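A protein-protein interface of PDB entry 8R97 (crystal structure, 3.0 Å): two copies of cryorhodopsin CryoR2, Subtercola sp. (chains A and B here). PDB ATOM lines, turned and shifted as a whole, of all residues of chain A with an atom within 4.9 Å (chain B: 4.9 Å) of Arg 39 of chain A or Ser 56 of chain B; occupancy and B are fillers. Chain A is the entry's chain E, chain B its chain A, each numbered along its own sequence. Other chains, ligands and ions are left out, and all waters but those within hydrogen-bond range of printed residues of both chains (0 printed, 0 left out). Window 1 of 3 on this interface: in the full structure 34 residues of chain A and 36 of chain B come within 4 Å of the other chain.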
ATOM      1  N   ALA A  35     -12.189 -22.450  24.455  1.00  0.00           N
ATOM      2  CA  ALA A  35     -12.374 -21.128  23.813  1.00  0.00           C
ATOM      3  C   ALA A  35     -11.020 -20.642  23.288  1.00  0.00           C
ATOM      4  O   ALA A  35     -10.954 -20.212  22.119  1.00  0.00           O
ATOM      5  CB  ALA A  35     -12.967 -20.151  24.798  1.00  0.00           C
ATOM      6  N   GLY A  36      -9.989 -20.718  24.135  1.00  0.00           N
ATOM      7  CA  GLY A  36      -8.605 -20.335  23.796  1.00  0.00           C
ATOM      8  C   GLY A  36      -8.075 -21.172  22.648  1.00  0.00           C
ATOM      9  O   GLY A  36      -7.592 -20.582  21.662  1.00  0.00           O
ATOM     10  N   PHE A  37      -8.176 -22.500  22.768  1.00  0.00           N
ATOM     11  CA  PHE A  37      -7.714 -23.486  21.755  1.00  0.00           C
ATOM     12  C   PHE A  37      -8.348 -23.157  20.399  1.00  0.00           C
ATOM     13  O   PHE A  37      -7.619 -23.086  19.386  1.00  0.00           O
ATOM     14  CB  PHE A  37      -8.058 -24.916  22.182  1.00  0.00           C
ATOM     15  CG  PHE A  37      -7.569 -25.977  21.228  1.00  0.00           C
ATOM     16  CD1 PHE A  37      -6.360 -26.618  21.437  1.00  0.00           C
ATOM     17  CD2 PHE A  37      -8.309 -26.315  20.105  1.00  0.00           C
ATOM     18  CE1 PHE A  37      -5.908 -27.586  20.553  1.00  0.00           C
ATOM     19  CE2 PHE A  37      -7.856 -27.282  19.221  1.00  0.00           C
ATOM     20  CZ  PHE A  37      -6.657 -27.915  19.447  1.00  0.00           C
ATOM     21  N   ILE A  38      -9.669 -22.961  20.386  1.00  0.00           N
ATOM     22  CA  ILE A  38     -10.456 -22.648  19.157  1.00  0.00           C
ATOM     23  C   ILE A  38      -9.905 -21.365  18.527  1.00  0.00           C
ATOM     24  O   ILE A  38      -9.577 -21.394  17.325  1.00  0.00           O
ATOM     25  CB  ILE A  38     -11.960 -22.536  19.471  1.00  0.00           C
ATOM     26  CG1 ILE A  38     -12.534 -23.880  19.926  1.00  0.00           C
ATOM     27  CG2 ILE A  38     -12.715 -21.977  18.273  1.00  0.00           C
ATOM     28  CD1 ILE A  38     -14.014 -23.853  20.221  1.00  0.00           C
ATOM     29  N   ARG A  39      -9.810 -20.286  19.308  1.00  0.00           N
ATOM     30  CA  ARG A  39      -9.289 -18.978  18.837  1.00  0.00           C
ATOM     31  C   ARG A  39      -7.901 -19.186  18.228  1.00  0.00           C
ATOM     32  O   ARG A  39      -7.714 -18.816  17.055  1.00  0.00           O
ATOM     33  CB  ARG A  39      -9.212 -17.961  19.978  1.00  0.00           C
ATOM     34  CG  ARG A  39      -8.875 -16.552  19.517  1.00  0.00           C
ATOM     35  CD  ARG A  39      -9.189 -15.554  20.614  1.00  0.00           C
ATOM     36  NE  ARG A  39      -8.856 -14.179  20.270  1.00  0.00           N
ATOM     37  CZ  ARG A  39      -9.099 -13.134  21.054  1.00  0.00           C
ATOM     38  NH1 ARG A  39      -9.683 -13.306  22.228  1.00  0.00           N
ATOM     39  NH2 ARG A  39      -8.763 -11.919  20.660  1.00  0.00           N
ATOM     40  N   THR A  40      -6.978 -19.768  18.999  1.00  0.00           N
ATOM     41  CA  THR A  40      -5.568 -20.026  18.599  1.00  0.00           C
ATOM     42  C   THR A  40      -5.530 -20.700  17.223  1.00  0.00           C
ATOM     43  O   THR A  40      -4.750 -20.238  16.365  1.00  0.00           O
ATOM     44  CB  THR A  40      -4.835 -20.880  19.640  1.00  0.00           C
ATOM     45  OG1 THR A  40      -4.725 -20.120  20.842  1.00  0.00           O
ATOM     46  CG2 THR A  40      -3.454 -21.301  19.190  1.00  0.00           C
ATOM     47  N   TYR A  41      -6.342 -21.745  17.031  1.00  0.00           N
ATOM     48  CA  TYR A  41      -6.405 -22.551  15.783  1.00  0.00           C
ATOM     49  C   TYR A  41      -6.858 -21.671  14.612  1.00  0.00           C
ATOM     50  O   TYR A  41      -6.191 -21.688  13.561  1.00  0.00           O
ATOM     51  CB  TYR A  41      -7.333 -23.756  15.953  1.00  0.00           C
ATOM     52  CG  TYR A  41      -7.428 -24.633  14.729  1.00  0.00           C
ATOM     53  CD1 TYR A  41      -8.474 -24.500  13.831  1.00  0.00           C
ATOM     54  CD2 TYR A  41      -6.456 -25.581  14.452  1.00  0.00           C
ATOM     55  CE1 TYR A  41      -8.561 -25.293  12.700  1.00  0.00           C
ATOM     56  CE2 TYR A  41      -6.528 -26.382  13.325  1.00  0.00           C
ATOM     57  CZ  TYR A  41      -7.584 -26.238  12.444  1.00  0.00           C
ATOM     58  OH  TYR A  41      -7.662 -27.025  11.332  1.00  0.00           O
ATOM     59  N   ILE A  42      -7.954 -20.928  14.789  1.00  0.00           N
ATOM     60  CA  ILE A  42      -8.568 -20.064  13.736  1.00  0.00           C
ATOM     61  C   ILE A  42      -7.605 -18.934  13.350  1.00  0.00           C
ATOM     62  O   ILE A  42      -7.573 -18.573  12.159  1.00  0.00           O
ATOM     63  CB  ILE A  42      -9.931 -19.515  14.200  1.00  0.00           C
ATOM     64  CG1 ILE A  42     -11.007 -20.602  14.168  1.00  0.00           C
ATOM     65  CG2 ILE A  42     -10.333 -18.301  13.377  1.00  0.00           C
ATOM     66  CD1 ILE A  42     -12.412 -20.063  14.058  1.00  0.00           C
ATOM     67  N   THR A  43      -6.861 -18.395  14.321  1.00  0.00           N
ATOM     68  CA  THR A  43      -5.909 -17.266  14.136  1.00  0.00           C
ATOM     69  C   THR A  43      -4.479 -17.805  14.027  1.00  0.00           C
ATOM     70  O   THR A  43      -3.557 -17.142  14.552  1.00  0.00           O
ATOM     71  CB  THR A  43      -6.017 -16.263  15.292  1.00  0.00           C
ATOM     72  OG1 THR A  43      -5.572 -16.907  16.486  1.00  0.00           O
ATOM     73  CG2 THR A  43      -7.424 -15.744  15.498  1.00  0.00           C
ATOM     74  N   ARG B  52     -11.876 -10.962  12.286  1.00  0.00           N
ATOM     75  CA  ARG B  52     -11.763 -12.420  12.567  1.00  0.00           C
ATOM     76  C   ARG B  52     -12.044 -12.688  14.048  1.00  0.00           C
ATOM     77  O   ARG B  52     -12.509 -13.801  14.363  1.00  0.00           O
ATOM     78  CB  ARG B  52     -10.383 -12.950  12.170  1.00  0.00           C
ATOM     79  CG  ARG B  52     -10.226 -14.455  12.344  1.00  0.00           C
ATOM     80  CD  ARG B  52      -9.005 -14.967  11.608  1.00  0.00           C
ATOM     81  NE  ARG B  52      -9.091 -14.655  10.188  1.00  0.00           N
ATOM     82  CZ  ARG B  52      -8.049 -14.537   9.373  1.00  0.00           C
ATOM     83  NH1 ARG B  52      -6.820 -14.686   9.837  1.00  0.00           N
ATOM     84  NH2 ARG B  52      -8.242 -14.248   8.099  1.00  0.00           N
ATOM     85  N   THR B  53     -11.768 -11.714  14.921  1.00  0.00           N
ATOM     86  CA  THR B  53     -12.011 -11.816  16.385  1.00  0.00           C
ATOM     87  C   THR B  53     -13.486 -12.171  16.602  1.00  0.00           C
ATOM     88  O   THR B  53     -13.778 -12.948  17.528  1.00  0.00           O
ATOM     89  CB  THR B  53     -11.621 -10.525  17.117  1.00  0.00           C
ATOM     90  OG1 THR B  53     -10.338 -10.107  16.654  1.00  0.00           O
ATOM     91  CG2 THR B  53     -11.593 -10.690  18.620  1.00  0.00           C
ATOM     92  N   ALA B  54     -14.370 -11.628  15.758  1.00  0.00           N
ATOM     93  CA  ALA B  54     -15.833 -11.850  15.792  1.00  0.00           C
ATOM     94  C   ALA B  54     -16.129 -13.336  15.561  1.00  0.00           C
ATOM     95  O   ALA B  54     -17.023 -13.876  16.240  1.00  0.00           O
ATOM     96  CB  ALA B  54     -16.509 -10.988  14.753  1.00  0.00           C
ATOM     97  N   VAL B  55     -15.394 -13.966  14.640  1.00  0.00           N
ATOM     98  CA  VAL B  55     -15.562 -15.400  14.259  1.00  0.00           C
ATOM     99  C   VAL B  55     -15.025 -16.285  15.388  1.00  0.00           C
ATOM    100  O   VAL B  55     -15.786 -17.142  15.881  1.00  0.00           O
ATOM    101  CB  VAL B  55     -14.859 -15.711  12.924  1.00  0.00           C
ATOM    102  CG1 VAL B  55     -14.992 -17.179  12.548  1.00  0.00           C
ATOM    103  CG2 VAL B  55     -15.367 -14.825  11.801  1.00  0.00           C
ATOM    104  N   SER B  56     -13.760 -16.087  15.773  1.00  0.00           N
ATOM    105  CA  SER B  56     -13.064 -16.863  16.833  1.00  0.00           C
ATOM    106  C   SER B  56     -13.906 -16.865  18.113  1.00  0.00           C
ATOM    107  O   SER B  56     -14.034 -17.937  18.735  1.00  0.00           O
ATOM    108  CB  SER B  56     -11.678 -16.328  17.080  1.00  0.00           C
ATOM    109  OG  SER B  56     -11.719 -14.948  17.406  1.00  0.00           O
ATOM    110  N   ALA B  57     -14.461 -15.708  18.484  1.00  0.00           N
ATOM    111  CA  ALA B  57     -15.307 -15.522  19.686  1.00  0.00           C
ATOM    112  C   ALA B  57     -16.583 -16.359  19.549  1.00  0.00           C
ATOM    113  O   ALA B  57     -16.891 -17.120  20.482  1.00  0.00           O
ATOM    114  CB  ALA B  57     -15.619 -14.060  19.871  1.00  0.00           C
ATOM    115  N   ARG B  58     -17.287 -16.227  18.419  1.00  0.00           N
ATOM    116  CA  ARG B  58     -18.553 -16.954  18.128  1.00  0.00           C
ATOM    117  C   ARG B  58     -18.290 -18.462  18.223  1.00  0.00           C
ATOM    118  O   ARG B  58     -18.930 -19.127  19.061  1.00  0.00           O
ATOM    119  CB  ARG B  58     -19.089 -16.555  16.749  1.00  0.00           C
ATOM    120  CG  ARG B  58     -20.391 -17.235  16.353  1.00  0.00           C
ATOM    121  CD  ARG B  58     -21.097 -16.554  15.191  1.00  0.00           C
ATOM    122  NE  ARG B  58     -20.264 -16.297  14.020  1.00  0.00           N
ATOM    123  CZ  ARG B  58     -19.783 -15.105  13.670  1.00  0.00           C
ATOM    124  NH1 ARG B  58     -20.051 -14.034  14.398  1.00  0.00           N
ATOM    125  NH2 ARG B  58     -19.041 -14.988  12.585  1.00  0.00           N
ATOM    126  N   LEU B  59     -17.368 -18.972  17.402  1.00  0.00           N
ATOM    127  CA  LEU B  59     -17.007 -20.413  17.367  1.00  0.00           C
ATOM    128  C   LEU B  59     -16.629 -20.859  18.784  1.00  0.00           C
ATOM    129  O   LEU B  59     -17.045 -21.958  19.196  1.00  0.00           O
ATOM    130  CB  LEU B  59     -15.851 -20.624  16.385  1.00  0.00           C
ATOM    131  CG  LEU B  59     -15.629 -22.070  15.945  1.00  0.00           C
ATOM    132  CD1 LEU B  59     -16.885 -22.633  15.299  1.00  0.00           C
ATOM    133  CD2 LEU B  59     -14.452 -22.180  14.991  1.00  0.00           C
ATOM    134  N   GLY B  60     -15.873 -20.022  19.497  1.00  0.00           N
ATOM    135  CA  GLY B  60     -15.439 -20.275  20.883  1.00  0.00           C
ATOM    136  C   GLY B  60     -16.628 -20.480  21.804  1.00  0.00           C
ATOM    137  O   GLY B  60     -16.656 -21.503  22.512  1.00  0.00           O
ATOM    138  N   ILE B 113     -17.075  -9.738  23.617  1.00  0.00           N
ATOM    139  CA  ILE B 113     -15.897  -9.611  22.708  1.00  0.00           C
ATOM    140  C   ILE B 113     -16.392  -9.666  21.260  1.00  0.00           C
ATOM    141  O   ILE B 113     -15.920  -8.854  20.441  1.00  0.00           O
ATOM    142  CB  ILE B 113     -14.859 -10.714  22.995  1.00  0.00           C
ATOM    143  CG1 ILE B 113     -14.576 -10.851  24.494  1.00  0.00           C
ATOM    144  CG2 ILE B 113     -13.586 -10.468  22.201  1.00  0.00           C
ATOM    145  CD1 ILE B 113     -13.672 -12.009  24.845  1.00  0.00           C
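Hydrophobic or aromatic side chains of chain A within 4 Å of the printed part of chain B: Ile 38 and Ile 42.
Of the 10 printed residues of chain B, 5 touch a printed residue of chain A.
Printed residues of chain B that touch a printed residue of chain A: Arg 52, Thr 53, Ser 56, Leu 59 and Gly 60.
Hydrophobic or aromatic side chains of chain B that line the printed part of chain A: Leu 59.
Among the printed residues, 6 pairs touch across the chains.
Among the printed residues, no Asp or Glu carboxylate lies within 4 Å of a Lys or Arg side-chain nitrogen of the other chain.
No position is printed for both chains.
Of the 6 pairs that touch across the chains among the printed residues, none has its exchanged pair printed and touching as well.
Leu 59 of chain B touches Ile 38 of chain A (O to CD1, 3.7 Å).
Gly 60 of chain B touches Ile 38 of chain A (CA to CD1, 3.9 Å).
Arg 39 of chain A touches Thr 53 of chain B (NH2 to CG2, 3.7 Å).
Arg 39 of chain A touches Ser 56 of chain B (CG to CB, 3.7 Å).
Ile 42 of chain A touches Arg 52 of chain B.
Ile 42 of chain A touches Leu 59 of chain B.
O of Arg 39 of chain A is in hydrogen-bond range of OG1 of Thr 43 of chain A.
OG of Ser 56 of chain B lies within hydrogen-bond range of O of Arg 52 of chain B, at 3.3 Å.
The side-chain hydroxyl of Ser 56 of chain B is in hydrogen-bond range of the backbone carbonyl oxygen of Thr 53 of chain B, 2.9 Å away.
Of the printed residues of chain B, Ile 38 of chain A touches Leu 59 and Gly 60.
Of the printed residues of chain A, Arg 52 of chain B touches Ile 42.
Of chain A, only Arg 39 comes within 4 Å of Ser 56 of chain B.
Of the printed residues of chain A, Leu 59 of chain B touches Ile 38 and Ile 42.
Ile 113 of chain B touches none of the printed residues of chain A.
The nearest residue of chain B that does not touch Arg 39 of chain A is Ile 113 of chain B (4.8 Å).
The nearest printed residue of chain A that does not touch Gly 60 of chain B is Ala 35 of chain A (4.3 Å).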
